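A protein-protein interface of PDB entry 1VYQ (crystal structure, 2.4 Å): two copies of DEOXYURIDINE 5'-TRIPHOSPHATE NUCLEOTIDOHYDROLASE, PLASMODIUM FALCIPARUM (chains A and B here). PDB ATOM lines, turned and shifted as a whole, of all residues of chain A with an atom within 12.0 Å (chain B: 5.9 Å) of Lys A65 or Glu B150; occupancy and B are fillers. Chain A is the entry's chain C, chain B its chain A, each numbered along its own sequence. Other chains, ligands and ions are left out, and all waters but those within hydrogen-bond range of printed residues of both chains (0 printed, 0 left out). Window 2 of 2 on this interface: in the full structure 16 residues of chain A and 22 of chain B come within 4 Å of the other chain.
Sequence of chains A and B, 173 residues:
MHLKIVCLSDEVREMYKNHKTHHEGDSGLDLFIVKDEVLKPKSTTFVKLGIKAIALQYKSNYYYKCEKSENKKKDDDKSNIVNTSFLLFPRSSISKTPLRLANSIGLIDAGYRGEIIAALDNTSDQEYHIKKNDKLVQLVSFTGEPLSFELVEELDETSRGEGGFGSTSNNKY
Hydrophobic or aromatic side chains of chain A that line the printed part of chain B: Tyr A63 and Tyr A64.
Of the 11 printed residues of chain B, 4 touch a printed residue of chain A.
Printed residues of chain B that touch a printed residue of chain A: Met B1, His B2, Ser B148 and Glu B150.
Hydrophobic or aromatic side chains of chain B that line the printed part of chain A: His B2.
Along chain B the printed residues that touch a printed residue of chain A span positions 1 to 150.
The backbone carbonyl oxygen (O) of Met B1 sits at hydrogen-bond distance from the backbone NH (N) of Ser B148 (2.8 Å).
ND1 of His B2 is in hydrogen-bond range of OG of Ser B148 (2.4 Å).
A ring nitrogen (NE2) of His B2 sits close to the side-chain carboxylate (OE2) of Glu B150 (3.1 Å).
O of Ser B148 sits at hydrogen-bond distance from N of Leu B3, at 2.7 Å.
The backbone carbonyl oxygen of Leu B3 is in hydrogen-bond range of the backbone NH of Glu B150 (3.0 Å).
N of Ile B5 is in hydrogen-bond range of O of Glu B150 (2.9 Å).
No position is printed for both chains.
Of the 6 pairs that touch across the chains among the printed residues, none has its exchanged pair printed and touching as well.
Of the printed residues of chain B, Lys A65 touches His B2, Ser B148 and Glu B150.
Of the printed residues of chain A, Glu B150 touches Lys A65.
Of the printed residues of chain A, His B2 touches Tyr A63 (3.7 Å) and Lys A65 (3.2 Å).
No residue of chain A comes within 4 Å of Ile B5.
No residue of chain A comes within 4 Å of Phe B149.
Leu B151 touches none of the printed residues of chain A.
No residue of chain A comes within 4 Å of Val B152.
Of the printed residues of chain B, Tyr A63 touches Met B1 (2.7 Å) and His B2 (3.7 Å).
Printed residues of chain A within 4 Å of Met B1: Tyr A63 (2.7 Å).
Of the printed residues of chain B, Tyr A64 touches Ser B148.
The nearest residue of chain B that does not touch Lys A65 is Phe B149 (5.3 Å).
The nearest residue of chain A that does not touch Glu B150 is Tyr A63 (5.8 Å).
N of Met B1 lies within hydrogen-bond range of O of Tyr A63 (2.7 Å).
OG of Ser B148 is in hydrogen-bond range of N of Lys A65, 3.1 Å away.
Among the printed residues, merely in contact across the chains: Tyr A63 with His B2 (3.7 Å), Tyr A64 with Ser B148 (3.7 Å), Lys A65 with His B2 (3.2 Å) and Lys A65 with Glu B150 (3.8 Å).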
ATOM      1  N   ASN A  61      -7.489 -27.800 -23.767  1.00  0.00           N
ATOM      2  CA  ASN A  61      -7.045 -26.539 -23.192  1.00  0.00           C
ATOM      3  C   ASN A  61      -5.931 -26.730 -22.147  1.00  0.00           C
ATOM      4  O   ASN A  61      -5.996 -27.587 -21.273  1.00  0.00           O
ATOM      5  CB  ASN A  61      -8.208 -25.656 -22.705  1.00  0.00           C
ATOM      6  CG  ASN A  61      -8.473 -24.453 -23.677  1.00  0.00           C
ATOM      7  OD1 ASN A  61      -7.582 -23.602 -23.896  1.00  0.00           O
ATOM      8  ND2 ASN A  61      -9.679 -24.409 -24.267  1.00  0.00           N
ATOM      9  N   TYR A  62      -4.896 -25.914 -22.326  1.00  0.00           N
ATOM     10  CA  TYR A  62      -3.687 -25.929 -21.528  1.00  0.00           C
ATOM     11  C   TYR A  62      -3.239 -24.493 -21.203  1.00  0.00           C
ATOM     12  O   TYR A  62      -3.502 -23.543 -21.963  1.00  0.00           O
ATOM     13  CB  TYR A  62      -2.577 -26.673 -22.287  1.00  0.00           C
ATOM     14  CG  TYR A  62      -2.275 -26.078 -23.655  1.00  0.00           C
ATOM     15  CD1 TYR A  62      -1.439 -24.954 -23.787  1.00  0.00           C
ATOM     16  CD2 TYR A  62      -2.813 -26.636 -24.816  1.00  0.00           C
ATOM     17  CE1 TYR A  62      -1.166 -24.399 -25.033  1.00  0.00           C
ATOM     18  CE2 TYR A  62      -2.544 -26.086 -26.056  1.00  0.00           C
ATOM     19  CZ  TYR A  62      -1.721 -24.966 -26.167  1.00  0.00           C
ATOM     20  OH  TYR A  62      -1.460 -24.410 -27.409  1.00  0.00           O
ATOM     21  N   TYR A  63      -2.559 -24.361 -20.063  1.00  0.00           N
ATOM     22  CA  TYR A  63      -1.984 -23.088 -19.620  1.00  0.00           C
ATOM     23  C   TYR A  63      -0.748 -22.616 -20.436  1.00  0.00           C
ATOM     24  O   TYR A  63       0.201 -23.358 -20.689  1.00  0.00           O
ATOM     25  CB  TYR A  63      -1.660 -23.169 -18.134  1.00  0.00           C
ATOM     26  CG  TYR A  63      -1.211 -21.869 -17.532  1.00  0.00           C
ATOM     27  CD1 TYR A  63      -0.146 -21.840 -16.640  1.00  0.00           C
ATOM     28  CD2 TYR A  63      -1.847 -20.663 -17.844  1.00  0.00           C
ATOM     29  CE1 TYR A  63       0.284 -20.654 -16.072  1.00  0.00           C
ATOM     30  CE2 TYR A  63      -1.414 -19.451 -17.286  1.00  0.00           C
ATOM     31  CZ  TYR A  63      -0.345 -19.462 -16.392  1.00  0.00           C
ATOM     32  OH  TYR A  63       0.114 -18.297 -15.811  1.00  0.00           O
ATOM     33  N   TYR A  64      -0.778 -21.361 -20.853  1.00  0.00           N
ATOM     34  CA  TYR A  64       0.255 -20.847 -21.755  1.00  0.00           C
ATOM     35  C   TYR A  64       0.316 -19.313 -21.703  1.00  0.00           C
ATOM     36  O   TYR A  64      -0.577 -18.662 -22.203  1.00  0.00           O
ATOM     37  CB  TYR A  64      -0.050 -21.323 -23.188  1.00  0.00           C
ATOM     38  CG  TYR A  64       1.026 -21.006 -24.200  1.00  0.00           C
ATOM     39  CD1 TYR A  64       1.083 -19.741 -24.855  1.00  0.00           C
ATOM     40  CD2 TYR A  64       1.982 -21.966 -24.522  1.00  0.00           C
ATOM     41  CE1 TYR A  64       2.105 -19.459 -25.804  1.00  0.00           C
ATOM     42  CE2 TYR A  64       2.988 -21.712 -25.462  1.00  0.00           C
ATOM     43  CZ  TYR A  64       3.057 -20.466 -26.097  1.00  0.00           C
ATOM     44  OH  TYR A  64       4.075 -20.290 -26.996  1.00  0.00           O
ATOM     45  N   LYS A  65       1.348 -18.762 -21.063  1.00  0.00           N
ATOM     46  CA  LYS A  65       1.633 -17.306 -21.055  1.00  0.00           C
ATOM     47  C   LYS A  65       2.370 -16.859 -22.322  1.00  0.00           C
ATOM     48  O   LYS A  65       3.122 -17.600 -22.938  1.00  0.00           O
ATOM     49  CB  LYS A  65       2.473 -16.986 -19.820  1.00  0.00           C
ATOM     50  CG  LYS A  65       1.755 -16.026 -18.868  1.00  0.00           C
ATOM     51  CD  LYS A  65       2.687 -15.464 -17.793  1.00  0.00           C
ATOM     52  N   MET B   1       1.710 -25.599 -21.071  1.00  0.00           N
ATOM     53  CA  MET B   1       2.388 -25.527 -19.746  1.00  0.00           C
ATOM     54  C   MET B   1       3.306 -24.310 -19.717  1.00  0.00           C
ATOM     55  O   MET B   1       3.846 -23.881 -20.754  1.00  0.00           O
ATOM     56  CB  MET B   1       3.163 -26.843 -19.474  1.00  0.00           C
ATOM     57  CG  MET B   1       4.102 -26.880 -18.244  1.00  0.00           C
ATOM     58  SD  MET B   1       5.045 -28.486 -18.106  1.00  0.00           S
ATOM     59  CE  MET B   1       6.706 -27.978 -18.647  1.00  0.00           C
ATOM     60  N   HIS B   2       3.475 -23.739 -18.528  1.00  0.00           N
ATOM     61  CA  HIS B   2       4.245 -22.522 -18.384  1.00  0.00           C
ATOM     62  C   HIS B   2       5.306 -22.717 -17.303  1.00  0.00           C
ATOM     63  O   HIS B   2       5.021 -23.195 -16.202  1.00  0.00           O
ATOM     64  CB  HIS B   2       3.323 -21.355 -18.060  1.00  0.00           C
ATOM     65  CG  HIS B   2       4.011 -20.039 -18.030  1.00  0.00           C
ATOM     66  ND1 HIS B   2       4.642 -19.507 -19.132  1.00  0.00           N
ATOM     67  CD2 HIS B   2       4.204 -19.155 -17.021  1.00  0.00           C
ATOM     68  CE1 HIS B   2       5.219 -18.363 -18.804  1.00  0.00           C
ATOM     69  NE2 HIS B   2       4.946 -18.112 -17.533  1.00  0.00           N
ATOM     70  N   LEU B   3       6.535 -22.334 -17.646  1.00  0.00           N
ATOM     71  CA  LEU B   3       7.686 -22.502 -16.788  1.00  0.00           C
ATOM     72  C   LEU B   3       8.065 -21.136 -16.287  1.00  0.00           C
ATOM     73  O   LEU B   3       8.136 -20.179 -17.057  1.00  0.00           O
ATOM     74  CB  LEU B   3       8.845 -23.069 -17.598  1.00  0.00           C
ATOM     75  CG  LEU B   3       8.583 -24.508 -17.999  1.00  0.00           C
ATOM     76  CD1 LEU B   3       9.395 -24.874 -19.206  1.00  0.00           C
ATOM     77  CD2 LEU B   3       8.783 -25.491 -16.808  1.00  0.00           C
ATOM     78  N   LYS B   4       8.280 -21.018 -14.987  1.00  0.00           N
ATOM     79  CA  LYS B   4       8.912 -19.820 -14.457  1.00  0.00           C
ATOM     80  C   LYS B   4      10.284 -20.264 -14.110  1.00  0.00           C
ATOM     81  O   LYS B   4      10.445 -21.316 -13.521  1.00  0.00           O
ATOM     82  CB  LYS B   4       8.183 -19.318 -13.241  1.00  0.00           C
ATOM     83  CG  LYS B   4       6.931 -18.520 -13.567  1.00  0.00           C
ATOM     84  CD  LYS B   4       6.180 -18.285 -12.276  1.00  0.00           C
ATOM     85  CE  LYS B   4       4.948 -17.391 -12.362  1.00  0.00           C
ATOM     86  NZ  LYS B   4       4.469 -17.194 -10.930  1.00  0.00           N
ATOM     87  N   ILE B   5      11.274 -19.474 -14.501  1.00  0.00           N
ATOM     88  CA  ILE B   5      12.642 -19.903 -14.462  1.00  0.00           C
ATOM     89  C   ILE B   5      13.560 -18.833 -13.893  1.00  0.00           C
ATOM     90  O   ILE B   5      13.520 -17.674 -14.357  1.00  0.00           O
ATOM     91  CB  ILE B   5      13.104 -20.218 -15.867  1.00  0.00           C
ATOM     92  CG1 ILE B   5      12.393 -21.472 -16.399  1.00  0.00           C
ATOM     93  CG2 ILE B   5      14.694 -20.360 -15.916  1.00  0.00           C
ATOM     94  CD1 ILE B   5      12.620 -21.690 -17.859  1.00  0.00           C
ATOM     95  N   VAL B   6      14.407 -19.259 -12.951  1.00  0.00           N
ATOM     96  CA  VAL B   6      15.429 -18.444 -12.326  1.00  0.00           C
ATOM     97  C   VAL B   6      16.738 -18.865 -12.896  1.00  0.00           C
ATOM     98  O   VAL B   6      17.127 -20.019 -12.748  1.00  0.00           O
ATOM     99  CB  VAL B   6      15.543 -18.705 -10.810  1.00  0.00           C
ATOM    100  CG1 VAL B   6      16.654 -17.899 -10.228  1.00  0.00           C
ATOM    101  CG2 VAL B   6      14.228 -18.412 -10.059  1.00  0.00           C
ATOM    102  N   SER B 148       5.457 -22.477 -22.562  1.00  0.00           N
ATOM    103  CA  SER B 148       5.885 -21.098 -22.414  1.00  0.00           C
ATOM    104  C   SER B 148       6.809 -20.965 -21.186  1.00  0.00           C
ATOM    105  O   SER B 148       6.821 -21.824 -20.309  1.00  0.00           O
ATOM    106  CB  SER B 148       4.673 -20.175 -22.248  1.00  0.00           C
ATOM    107  OG  SER B 148       3.854 -20.559 -21.157  1.00  0.00           O
ATOM    108  N   PHE B 149       7.580 -19.884 -21.142  1.00  0.00           N
ATOM    109  CA  PHE B 149       8.376 -19.571 -19.975  1.00  0.00           C
ATOM    110  C   PHE B 149       8.636 -18.071 -19.849  1.00  0.00           C
ATOM    111  O   PHE B 149       8.780 -17.357 -20.866  1.00  0.00           O
ATOM    112  CB  PHE B 149       9.706 -20.310 -20.009  1.00  0.00           C
ATOM    113  CG  PHE B 149      10.691 -19.742 -21.005  1.00  0.00           C
ATOM    114  CD1 PHE B 149      11.692 -18.866 -20.600  1.00  0.00           C
ATOM    115  CD2 PHE B 149      10.634 -20.093 -22.328  1.00  0.00           C
ATOM    116  CE1 PHE B 149      12.619 -18.320 -21.525  1.00  0.00           C
ATOM    117  CE2 PHE B 149      11.572 -19.593 -23.235  1.00  0.00           C
ATOM    118  CZ  PHE B 149      12.563 -18.683 -22.824  1.00  0.00           C
ATOM    119  N   GLU B 150       8.612 -17.615 -18.595  1.00  0.00           N
ATOM    120  CA  GLU B 150       9.223 -16.361 -18.223  1.00  0.00           C
ATOM    121  C   GLU B 150      10.434 -16.649 -17.337  1.00  0.00           C
ATOM    122  O   GLU B 150      10.503 -17.695 -16.668  1.00  0.00           O
ATOM    123  CB  GLU B 150       8.282 -15.420 -17.458  1.00  0.00           C
ATOM    124  CG  GLU B 150       6.993 -16.040 -16.988  1.00  0.00           C
ATOM    125  CD  GLU B 150       6.440 -15.466 -15.717  1.00  0.00           C
ATOM    126  OE1 GLU B 150       6.972 -14.483 -15.156  1.00  0.00           O
ATOM    127  OE2 GLU B 150       5.450 -16.024 -15.270  1.00  0.00           O
ATOM    128  N   LEU B 151      11.355 -15.690 -17.388  1.00  0.00           N
ATOM    129  CA  LEU B 151      12.459 -15.530 -16.477  1.00  0.00           C
ATOM    130  C   LEU B 151      11.983 -14.740 -15.272  1.00  0.00           C
ATOM    131  O   LEU B 151      11.089 -13.952 -15.360  1.00  0.00           O
ATOM    132  CB  LEU B 151      13.601 -14.798 -17.190  1.00  0.00           C
ATOM    133  CG  LEU B 151      14.107 -15.520 -18.442  1.00  0.00           C
ATOM    134  CD1 LEU B 151      15.432 -14.986 -18.851  1.00  0.00           C
ATOM    135  CD2 LEU B 151      14.223 -17.088 -18.199  1.00  0.00           C
ATOM    136  N   VAL B 152      12.572 -14.991 -14.122  1.00  0.00           N
ATOM    137  CA  VAL B 152      11.984 -14.566 -12.863  1.00  0.00           C
ATOM    138  C   VAL B 152      13.127 -14.506 -11.843  1.00  0.00           C
ATOM    139  O   VAL B 152      14.137 -15.220 -12.004  1.00  0.00           O
ATOM    140  CB  VAL B 152      10.827 -15.562 -12.489  1.00  0.00           C
ATOM    141  CG1 VAL B 152      10.838 -15.908 -11.118  1.00  0.00           C
ATOM    142  CG2 VAL B 152       9.420 -14.978 -12.863  1.00  0.00           C
